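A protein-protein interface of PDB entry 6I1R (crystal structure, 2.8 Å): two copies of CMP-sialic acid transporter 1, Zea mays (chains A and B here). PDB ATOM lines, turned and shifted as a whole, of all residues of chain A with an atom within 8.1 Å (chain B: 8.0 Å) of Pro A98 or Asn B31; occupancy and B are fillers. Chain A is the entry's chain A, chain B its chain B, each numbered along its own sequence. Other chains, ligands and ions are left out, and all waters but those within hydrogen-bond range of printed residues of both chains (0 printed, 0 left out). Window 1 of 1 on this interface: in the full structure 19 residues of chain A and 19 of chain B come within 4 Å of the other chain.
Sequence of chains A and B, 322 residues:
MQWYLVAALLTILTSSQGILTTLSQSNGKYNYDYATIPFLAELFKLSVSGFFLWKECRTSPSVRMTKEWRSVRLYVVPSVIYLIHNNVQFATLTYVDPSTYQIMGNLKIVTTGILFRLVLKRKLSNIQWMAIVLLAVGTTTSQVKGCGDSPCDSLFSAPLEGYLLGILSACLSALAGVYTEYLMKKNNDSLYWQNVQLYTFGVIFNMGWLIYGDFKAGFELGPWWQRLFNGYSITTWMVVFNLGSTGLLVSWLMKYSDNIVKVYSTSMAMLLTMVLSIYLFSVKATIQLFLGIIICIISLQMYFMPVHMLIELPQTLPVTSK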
ATOM      1  N   THR A  92       2.408  20.754  22.319  1.00  0.00           N
ATOM      2  CA  THR A  92       2.575  22.199  22.102  1.00  0.00           C
ATOM      3  C   THR A  92       2.423  22.531  20.613  1.00  0.00           C
ATOM      4  O   THR A  92       1.588  23.354  20.236  1.00  0.00           O
ATOM      5  CB  THR A  92       3.936  22.692  22.615  1.00  0.00           C
ATOM      6  OG1 THR A  92       4.186  22.106  23.892  1.00  0.00           O
ATOM      7  CG2 THR A  92       4.011  24.198  22.733  1.00  0.00           C
ATOM      8  N   LEU A  93       3.207  21.852  19.776  1.00  0.00           N
ATOM      9  CA  LEU A  93       3.297  22.150  18.339  1.00  0.00           C
ATOM     10  C   LEU A  93       1.928  22.037  17.650  1.00  0.00           C
ATOM     11  O   LEU A  93       1.798  22.460  16.502  1.00  0.00           O
ATOM     12  CB  LEU A  93       4.307  21.193  17.694  1.00  0.00           C
ATOM     13  CG  LEU A  93       5.775  21.455  18.031  1.00  0.00           C
ATOM     14  CD1 LEU A  93       6.622  20.220  17.765  1.00  0.00           C
ATOM     15  CD2 LEU A  93       6.310  22.652  17.257  1.00  0.00           C
ATOM     16  N   THR A  94       0.918  21.476  18.315  1.00  0.00           N
ATOM     17  CA  THR A  94      -0.430  21.422  17.733  1.00  0.00           C
ATOM     18  C   THR A  94      -1.216  22.697  18.075  1.00  0.00           C
ATOM     19  O   THR A  94      -2.374  22.815  17.683  1.00  0.00           O
ATOM     20  CB  THR A  94      -1.195  20.161  18.163  1.00  0.00           C
ATOM     21  OG1 THR A  94      -1.601  20.286  19.527  1.00  0.00           O
ATOM     22  CG2 THR A  94      -0.389  18.893  17.992  1.00  0.00           C
ATOM     23  N   TYR A  95      -0.609  23.639  18.799  1.00  0.00           N
ATOM     24  CA  TYR A  95      -1.216  24.957  19.017  1.00  0.00           C
ATOM     25  C   TYR A  95      -0.346  26.072  18.415  1.00  0.00           C
ATOM     26  O   TYR A  95      -0.881  27.120  18.053  1.00  0.00           O
ATOM     27  CB  TYR A  95      -1.436  25.214  20.509  1.00  0.00           C
ATOM     28  CG  TYR A  95      -2.396  24.267  21.185  1.00  0.00           C
ATOM     29  CD1 TYR A  95      -1.961  23.054  21.693  1.00  0.00           C
ATOM     30  CD2 TYR A  95      -3.736  24.586  21.331  1.00  0.00           C
ATOM     31  CE1 TYR A  95      -2.831  22.180  22.324  1.00  0.00           C
ATOM     32  CE2 TYR A  95      -4.622  23.723  21.959  1.00  0.00           C
ATOM     33  CZ  TYR A  95      -4.168  22.514  22.456  1.00  0.00           C
ATOM     34  OH  TYR A  95      -5.031  21.657  23.075  1.00  0.00           O
ATOM     35  N   VAL A  96       0.969  25.869  18.306  1.00  0.00           N
ATOM     36  CA  VAL A  96       1.877  26.944  17.887  1.00  0.00           C
ATOM     37  C   VAL A  96       2.719  26.472  16.695  1.00  0.00           C
ATOM     38  O   VAL A  96       3.042  25.290  16.572  1.00  0.00           O
ATOM     39  CB  VAL A  96       2.780  27.413  19.045  1.00  0.00           C
ATOM     40  CG1 VAL A  96       1.968  27.973  20.203  1.00  0.00           C
ATOM     41  CG2 VAL A  96       3.719  26.317  19.531  1.00  0.00           C
ATOM     42  N   ASP A  97       3.073  27.422  15.830  1.00  0.00           N
ATOM     43  CA  ASP A  97       4.062  27.183  14.777  1.00  0.00           C
ATOM     44  C   ASP A  97       5.417  26.903  15.442  1.00  0.00           C
ATOM     45  O   ASP A  97       5.658  27.366  16.557  1.00  0.00           O
ATOM     46  CB  ASP A  97       4.138  28.359  13.795  1.00  0.00           C
ATOM     47  CG  ASP A  97       4.243  29.728  14.450  1.00  0.00           C
ATOM     48  OD1 ASP A  97       5.135  29.907  15.301  1.00  0.00           O
ATOM     49  OD2 ASP A  97       3.430  30.609  14.097  1.00  0.00           O
ATOM     50  N   PRO A  98       6.303  26.145  14.766  1.00  0.00           N
ATOM     51  CA  PRO A  98       7.604  25.778  15.353  1.00  0.00           C
ATOM     52  C   PRO A  98       8.495  26.975  15.728  1.00  0.00           C
ATOM     53  O   PRO A  98       9.346  26.837  16.606  1.00  0.00           O
ATOM     54  CB  PRO A  98       8.304  24.932  14.278  1.00  0.00           C
ATOM     55  CG  PRO A  98       7.164  24.366  13.479  1.00  0.00           C
ATOM     56  CD  PRO A  98       6.156  25.493  13.455  1.00  0.00           C
ATOM     57  N   SER A  99       8.314  28.124  15.075  1.00  0.00           N
ATOM     58  CA  SER A  99       9.091  29.324  15.408  1.00  0.00           C
ATOM     59  C   SER A  99       8.694  29.834  16.800  1.00  0.00           C
ATOM     60  O   SER A  99       9.559  30.071  17.646  1.00  0.00           O
ATOM     61  CB  SER A  99       8.926  30.393  14.355  1.00  0.00           C
ATOM     62  OG  SER A  99       7.554  30.625  14.074  1.00  0.00           O
ATOM     63  N   THR A 100       7.392  29.986  17.031  1.00  0.00           N
ATOM     64  CA  THR A 100       6.869  30.373  18.347  1.00  0.00           C
ATOM     65  C   THR A 100       7.382  29.394  19.412  1.00  0.00           C
ATOM     66  O   THR A 100       7.773  29.803  20.503  1.00  0.00           O
ATOM     67  CB  THR A 100       5.336  30.442  18.329  1.00  0.00           C
ATOM     68  OG1 THR A 100       4.947  31.472  17.419  1.00  0.00           O
ATOM     69  CG2 THR A 100       4.729  30.719  19.688  1.00  0.00           C
ATOM     70  N   TYR A 101       7.381  28.107  19.073  1.00  0.00           N
ATOM     71  CA  TYR A 101       7.844  27.040  19.969  1.00  0.00           C
ATOM     72  C   TYR A 101       9.359  27.166  20.188  1.00  0.00           C
ATOM     73  O   TYR A 101       9.838  27.041  21.318  1.00  0.00           O
ATOM     74  CB  TYR A 101       7.414  25.681  19.403  1.00  0.00           C
ATOM     75  CG  TYR A 101       8.185  24.478  19.886  1.00  0.00           C
ATOM     76  CD1 TYR A 101       7.993  23.958  21.157  1.00  0.00           C
ATOM     77  CD2 TYR A 101       9.083  23.831  19.051  1.00  0.00           C
ATOM     78  CE1 TYR A 101       8.692  22.845  21.593  1.00  0.00           C
ATOM     79  CE2 TYR A 101       9.790  22.717  19.471  1.00  0.00           C
ATOM     80  CZ  TYR A 101       9.593  22.223  20.747  1.00  0.00           C
ATOM     81  OH  TYR A 101      10.291  21.126  21.156  1.00  0.00           O
ATOM     82  N   GLN A 102      10.103  27.430  19.115  1.00  0.00           N
ATOM     83  CA  GLN A 102      11.560  27.559  19.189  1.00  0.00           C
ATOM     84  C   GLN A 102      11.947  28.732  20.102  1.00  0.00           C
ATOM     85  O   GLN A 102      12.944  28.644  20.817  1.00  0.00           O
ATOM     86  CB  GLN A 102      12.154  27.756  17.793  1.00  0.00           C
ATOM     87  N   ILE A 103      11.162  29.811  20.086  1.00  0.00           N
ATOM     88  CA  ILE A 103      11.527  31.038  20.806  1.00  0.00           C
ATOM     89  C   ILE A 103      11.055  30.951  22.265  1.00  0.00           C
ATOM     90  O   ILE A 103      11.678  31.545  23.145  1.00  0.00           O
ATOM     91  CB  ILE A 103      10.992  32.293  20.079  1.00  0.00           C
ATOM     92  CG1 ILE A 103      11.827  33.533  20.411  1.00  0.00           C
ATOM     93  CG2 ILE A 103       9.514  32.525  20.361  1.00  0.00           C
ATOM     94  CD1 ILE A 103      11.773  34.613  19.354  1.00  0.00           C
ATOM     95  N   MET A 104       9.973  30.219  22.526  1.00  0.00           N
ATOM     96  CA  MET A 104       9.563  29.919  23.906  1.00  0.00           C
ATOM     97  C   MET A 104      10.618  29.028  24.578  1.00  0.00           C
ATOM     98  O   MET A 104      10.664  28.943  25.802  1.00  0.00           O
ATOM     99  CB  MET A 104       8.209  29.201  23.950  1.00  0.00           C
ATOM    100  CG  MET A 104       7.019  30.124  23.777  1.00  0.00           C
ATOM    101  SD  MET A 104       5.444  29.295  24.133  1.00  0.00           S
ATOM    102  CE  MET A 104       5.475  27.972  22.925  1.00  0.00           C
ATOM    103  N   GLY A 105      11.449  28.365  23.773  1.00  0.00           N
ATOM    104  CA  GLY A 105      12.502  27.476  24.266  1.00  0.00           C
ATOM    105  C   GLY A 105      13.541  28.185  25.124  1.00  0.00           C
ATOM    106  O   GLY A 105      14.217  27.542  25.918  1.00  0.00           O
ATOM    107  N   GLN A 143      16.384  35.545  17.880  1.00  0.00           N
ATOM    108  CA  GLN A 143      15.408  34.697  17.198  1.00  0.00           C
ATOM    109  C   GLN A 143      14.222  35.528  16.688  1.00  0.00           C
ATOM    110  O   GLN A 143      13.591  35.134  15.708  1.00  0.00           O
ATOM    111  CB  GLN A 143      14.926  33.586  18.134  1.00  0.00           C
ATOM    112  CG  GLN A 143      16.019  32.595  18.506  1.00  0.00           C
ATOM    113  CD  GLN A 143      15.460  31.315  19.076  1.00  0.00           C
ATOM    114  OE1 GLN A 143      15.361  31.143  20.289  1.00  0.00           O
ATOM    115  NE2 GLN A 143      15.075  30.404  18.196  1.00  0.00           N
ATOM    116  N   SER A 150       8.153  36.053   6.003  1.00  0.00           N
ATOM    117  CA  SER A 150       6.968  35.490   5.350  1.00  0.00           C
ATOM    118  C   SER A 150       6.022  34.822   6.360  1.00  0.00           C
ATOM    119  O   SER A 150       4.814  35.059   6.307  1.00  0.00           O
ATOM    120  CB  SER A 150       7.372  34.536   4.256  1.00  0.00           C
ATOM    121  N   PRO A 151       6.550  33.978   7.270  1.00  0.00           N
ATOM    122  CA  PRO A 151       5.663  33.417   8.288  1.00  0.00           C
ATOM    123  C   PRO A 151       5.448  34.430   9.424  1.00  0.00           C
ATOM    124  O   PRO A 151       6.139  34.383  10.444  1.00  0.00           O
ATOM    125  CB  PRO A 151       6.381  32.144   8.756  1.00  0.00           C
ATOM    126  CG  PRO A 151       7.840  32.492   8.627  1.00  0.00           C
ATOM    127  CD  PRO A 151       7.912  33.452   7.456  1.00  0.00           C
ATOM    128  N   CYS A 152       4.502  35.343   9.221  1.00  0.00           N
ATOM    129  CA  CYS A 152       4.201  36.388  10.204  1.00  0.00           C
ATOM    130  C   CYS A 152       3.474  35.778  11.409  1.00  0.00           C
ATOM    131  O   CYS A 152       2.261  35.566  11.369  1.00  0.00           O
ATOM    132  CB  CYS A 152       3.350  37.498   9.598  1.00  0.00           C
ATOM    133  SG  CYS A 152       4.255  38.561   8.442  1.00  0.00           S
ATOM    134  N   ASP A 153       4.227  35.499  12.471  1.00  0.00           N
ATOM    135  CA  ASP A 153       3.653  34.968  13.705  1.00  0.00           C
ATOM    136  C   ASP A 153       3.018  36.123  14.489  1.00  0.00           C
ATOM    137  O   ASP A 153       3.717  36.895  15.150  1.00  0.00           O
ATOM    138  CB  ASP A 153       4.708  34.235  14.539  1.00  0.00           C
ATOM    139  N   LEU B  23      11.624  24.795  -1.376  1.00  0.00           N
ATOM    140  CA  LEU B  23      12.002  26.117  -0.845  1.00  0.00           C
ATOM    141  C   LEU B  23      11.194  26.416   0.430  1.00  0.00           C
ATOM    142  O   LEU B  23      11.766  26.739   1.498  1.00  0.00           O
ATOM    143  CB  LEU B  23      11.765  27.185  -1.922  1.00  0.00           C
ATOM    144  CG  LEU B  23      12.790  27.231  -3.057  1.00  0.00           C
ATOM    145  CD1 LEU B  23      12.355  28.198  -4.149  1.00  0.00           C
ATOM    146  CD2 LEU B  23      14.169  27.612  -2.535  1.00  0.00           C
ATOM    147  N   SER B  24       9.870  26.290   0.314  1.00  0.00           N
ATOM    148  CA  SER B  24       8.947  26.514   1.431  1.00  0.00           C
ATOM    149  C   SER B  24       9.177  25.466   2.522  1.00  0.00           C
ATOM    150  O   SER B  24       8.992  25.740   3.711  1.00  0.00           O
ATOM    151  CB  SER B  24       7.515  26.478   0.977  1.00  0.00           C
ATOM    152  OG  SER B  24       7.010  25.162   0.982  1.00  0.00           O
ATOM    153  N   GLN B  25       9.567  24.272   2.088  1.00  0.00           N
ATOM    154  CA  GLN B  25       9.954  23.199   2.980  1.00  0.00           C
ATOM    155  C   GLN B  25      11.323  23.501   3.606  1.00  0.00           C
ATOM    156  O   GLN B  25      12.074  22.569   3.901  1.00  0.00           O
ATOM    157  CB  GLN B  25      10.011  21.877   2.211  1.00  0.00           C
ATOM    158  N   SER B  26      11.668  24.774   3.809  1.00  0.00           N
ATOM    159  CA  SER B  26      12.939  25.065   4.464  1.00  0.00           C
ATOM    160  C   SER B  26      12.809  24.859   5.982  1.00  0.00           C
ATOM    161  O   SER B  26      12.518  25.790   6.725  1.00  0.00           O
ATOM    162  CB  SER B  26      13.449  26.434   4.112  1.00  0.00           C
ATOM    163  OG  SER B  26      12.544  27.445   4.461  1.00  0.00           O
ATOM    164  N   ASN B  27      13.032  23.626   6.434  1.00  0.00           N
ATOM    165  CA  ASN B  27      12.757  23.240   7.821  1.00  0.00           C
ATOM    166  C   ASN B  27      11.273  23.484   8.129  1.00  0.00           C
ATOM    167  O   ASN B  27      10.396  23.195   7.310  1.00  0.00           O
ATOM    168  CB  ASN B  27      13.667  23.979   8.808  1.00  0.00           C
ATOM    169  N   ASN B  31       8.080  24.928   7.726  1.00  0.00           N
ATOM    170  CA  ASN B  31       7.665  25.608   8.955  1.00  0.00           C
ATOM    171  C   ASN B  31       6.181  25.334   9.250  1.00  0.00           C
ATOM    172  O   ASN B  31       5.661  25.804  10.263  1.00  0.00           O
ATOM    173  CB  ASN B  31       7.923  27.117   8.869  1.00  0.00           C
ATOM    174  CG  ASN B  31       8.443  27.707  10.164  1.00  0.00           C
ATOM    175  OD1 ASN B  31       9.529  27.353  10.619  1.00  0.00           O
ATOM    176  ND2 ASN B  31       7.686  28.616  10.755  1.00  0.00           N
ATOM    177  N   TYR B  32       5.511  24.557   8.397  1.00  0.00           N
ATOM    178  CA  TYR B  32       4.043  24.444   8.415  1.00  0.00           C
ATOM    179  C   TYR B  32       3.638  22.968   8.315  1.00  0.00           C
ATOM    180  O   TYR B  32       4.473  22.077   8.484  1.00  0.00           O
ATOM    181  CB  TYR B  32       3.453  25.267   7.267  1.00  0.00           C
ATOM    182  CG  TYR B  32       3.982  24.873   5.914  1.00  0.00           C
ATOM    183  CD1 TYR B  32       5.168  25.340   5.431  1.00  0.00           C
ATOM    184  CD2 TYR B  32       3.334  23.995   5.101  1.00  0.00           C
ATOM    185  CE1 TYR B  32       5.680  24.974   4.199  1.00  0.00           C
ATOM    186  CE2 TYR B  32       3.823  23.631   3.856  1.00  0.00           C
ATOM    187  CZ  TYR B  32       5.012  24.110   3.383  1.00  0.00           C
ATOM    188  OH  TYR B  32       5.515  23.751   2.166  1.00  0.00           O
ATOM    189  N   ASP B  33       2.356  22.729   8.042  1.00  0.00           N
ATOM    190  CA  ASP B  33       1.810  21.386   7.876  1.00  0.00           C
ATOM    191  C   ASP B  33       1.494  21.153   6.392  1.00  0.00           C
ATOM    192  O   ASP B  33       0.696  21.883   5.799  1.00  0.00           O
ATOM    193  CB  ASP B  33       0.558  21.200   8.742  1.00  0.00           C
ATOM    194  CG  ASP B  33       0.483  19.880   9.495  1.00  0.00           C
ATOM    195  OD1 ASP B  33       1.210  18.938   9.119  1.00  0.00           O
ATOM    196  OD2 ASP B  33      -0.313  19.801  10.452  1.00  0.00           O
ATOM    197  N   TYR B  34       2.108  20.123   5.809  1.00  0.00           N
ATOM    198  CA  TYR B  34       1.771  19.675   4.457  1.00  0.00           C
ATOM    199  C   TYR B  34       0.574  18.712   4.522  1.00  0.00           C
ATOM    200  O   TYR B  34       0.248  18.052   3.536  1.00  0.00           O
ATOM    201  CB  TYR B  34       3.001  19.042   3.793  1.00  0.00           C
ATOM    202  CG  TYR B  34       2.998  18.986   2.283  1.00  0.00           C
ATOM    203  CD1 TYR B  34       1.965  19.519   1.524  1.00  0.00           C
ATOM    204  CD2 TYR B  34       4.068  18.425   1.601  1.00  0.00           C
ATOM    205  CE1 TYR B  34       1.978  19.468   0.138  1.00  0.00           C
ATOM    206  CE2 TYR B  34       4.100  18.370   0.217  1.00  0.00           C
ATOM    207  CZ  TYR B  34       3.051  18.893  -0.519  1.00  0.00           C
ATOM    208  OH  TYR B  34       3.071  18.845  -1.883  1.00  0.00           O
ATOM    209  N   PHE B 229      -3.625  27.575   9.794  1.00  0.00           N
ATOM    210  CA  PHE B 229      -2.833  28.647   9.168  1.00  0.00           C
ATOM    211  C   PHE B 229      -1.403  28.688   9.727  1.00  0.00           C
ATOM    212  O   PHE B 229      -0.600  29.501   9.271  1.00  0.00           O
ATOM    213  CB  PHE B 229      -3.526  30.001   9.361  1.00  0.00           C
ATOM    214  CG  PHE B 229      -4.413  30.439   8.220  1.00  0.00           C
ATOM    215  CD1 PHE B 229      -5.290  29.552   7.613  1.00  0.00           C
ATOM    216  CD2 PHE B 229      -4.386  31.751   7.769  1.00  0.00           C
ATOM    217  CE1 PHE B 229      -6.104  29.963   6.568  1.00  0.00           C
ATOM    218  CE2 PHE B 229      -5.205  32.161   6.727  1.00  0.00           C
ATOM    219  CZ  PHE B 229      -6.063  31.266   6.129  1.00  0.00           C
ATOM    220  N   ASN B 230      -1.068  27.823  10.684  1.00  0.00           N
ATOM    221  CA  ASN B 230       0.216  27.930  11.394  1.00  0.00           C
ATOM    222  C   ASN B 230       1.384  27.779  10.409  1.00  0.00           C
ATOM    223  O   ASN B 230       1.349  26.943   9.504  1.00  0.00           O
ATOM    224  CB  ASN B 230       0.339  26.908  12.530  1.00  0.00           C
ATOM    225  CG  ASN B 230      -0.378  27.328  13.798  1.00  0.00           C
ATOM    226  OD1 ASN B 230      -0.539  28.515  14.069  1.00  0.00           O
ATOM    227  ND2 ASN B 230      -0.795  26.358  14.593  1.00  0.00           N
ATOM    228  N   GLY B 231       2.400  28.623  10.589  1.00  0.00           N
ATOM    229  CA  GLY B 231       3.656  28.531   9.843  1.00  0.00           C
ATOM    230  C   GLY B 231       3.531  28.966   8.390  1.00  0.00           C
ATOM    231  O   GLY B 231       4.527  28.943   7.661  1.00  0.00           O
ATOM    232  N   TYR B 232       2.336  29.385   7.970  1.00  0.00           N
ATOM    233  CA  TYR B 232       2.053  29.628   6.551  1.00  0.00           C
ATOM    234  C   TYR B 232       2.761  30.902   6.082  1.00  0.00           C
ATOM    235  O   TYR B 232       2.336  32.014   6.393  1.00  0.00           O
ATOM    236  CB  TYR B 232       0.545  29.726   6.294  1.00  0.00           C
ATOM    237  CG  TYR B 232      -0.104  28.431   5.879  1.00  0.00           C
ATOM    238  CD1 TYR B 232      -0.278  27.390   6.777  1.00  0.00           C
ATOM    239  CD2 TYR B 232      -0.541  28.242   4.577  1.00  0.00           C
ATOM    240  CE1 TYR B 232      -0.869  26.197   6.393  1.00  0.00           C
ATOM    241  CE2 TYR B 232      -1.135  27.056   4.179  1.00  0.00           C
ATOM    242  CZ  TYR B 232      -1.302  26.029   5.090  1.00  0.00           C
ATOM    243  OH  TYR B 232      -1.889  24.859   4.702  1.00  0.00           O
ATOM    244  N   SER B 233       3.839  30.715   5.327  1.00  0.00           N
ATOM    245  CA  SER B 233       4.558  31.819   4.703  1.00  0.00           C
ATOM    246  C   SER B 233       3.852  32.220   3.402  1.00  0.00           C
ATOM    247  O   SER B 233       2.815  31.651   3.049  1.00  0.00           O
ATOM    248  CB  SER B 233       5.996  31.442   4.456  1.00  0.00           C
ATOM    249  OG  SER B 233       6.077  30.241   3.709  1.00  0.00           O
ATOM    250  N   THR B 236       4.426  29.282   1.169  1.00  0.00           N
ATOM    251  CA  THR B 236       3.412  28.265   1.450  1.00  0.00           C
ATOM    252  C   THR B 236       2.160  28.544   0.607  1.00  0.00           C
ATOM    253  O   THR B 236       1.607  27.627   0.004  1.00  0.00           O
ATOM    254  CB  THR B 236       3.057  28.200   2.940  1.00  0.00           C
ATOM    255  OG1 THR B 236       4.257  28.275   3.711  1.00  0.00           O
ATOM    256  CG2 THR B 236       2.315  26.933   3.299  1.00  0.00           C
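OG of Ser A99 lies within hydrogen-bond range of OD1 of Asp A97, at 2.8 Å.
OD1 of Asp A97 lies within hydrogen-bond range of OG1 of Thr A100 (2.6 Å).
The side-chain hydroxyl (OG1) of Thr B236 is in hydrogen-bond range of the side-chain hydroxyl (OG) of Ser B233.
Of chain B, only Asn B31 (3.2 Å) comes within 4 Å of Pro A98.
Printed residues of chain A within 4 Å of Asn B31: Pro A98 and Ser A99.
Printed residues of chain A within 4 Å of Ser B233: Ser A150 and Pro A151.
Of the printed residues of chain B, Pro A151 touches Gly B231 (3.9 Å) and Ser B233 (3.8 Å).
Tyr B34 touches none of the printed residues of chain A.
Thr B236 touches none of the printed residues of chain A.
The nearest residue of chain A that does not touch Asn B31 is Pro A151 (4.3 Å).
Among the printed residues, pairs that only touch across the chains: Pro A98 with Asn B31, Ser A150 with Ser B233, Tyr A95 with Asn B230, Asp A97 with Gly B231, Pro A151 with Ser B233, Pro A151 with Gly B231, Ser A99 with Asn B31 and Ser A150 with Tyr B232.
No position is printed for both chains.
Of the 8 pairs that touch across the chains among the printed residues, none has its exchanged pair printed and touching as well.
Printed residues of chain A that touch a printed residue of chain B: Tyr A95, Asp A97, Pro A98, Ser A99, Ser A150 and Pro A151.
Hydrophobic or aromatic side chains of chain A within 4 Å of the printed part of chain B: Pro A98 and Pro A151.
Along chain A the printed residues that touch a printed residue of chain B span positions 95 to 151.
Printed residues of chain B that touch a printed residue of chain A: Asn B31, Asn B230, Gly B231, Tyr B232 and Ser B233.
Among the printed residues, no Asp or Glu carboxylate lies within 4 Å of a Lys or Arg side-chain nitrogen of the other chain.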
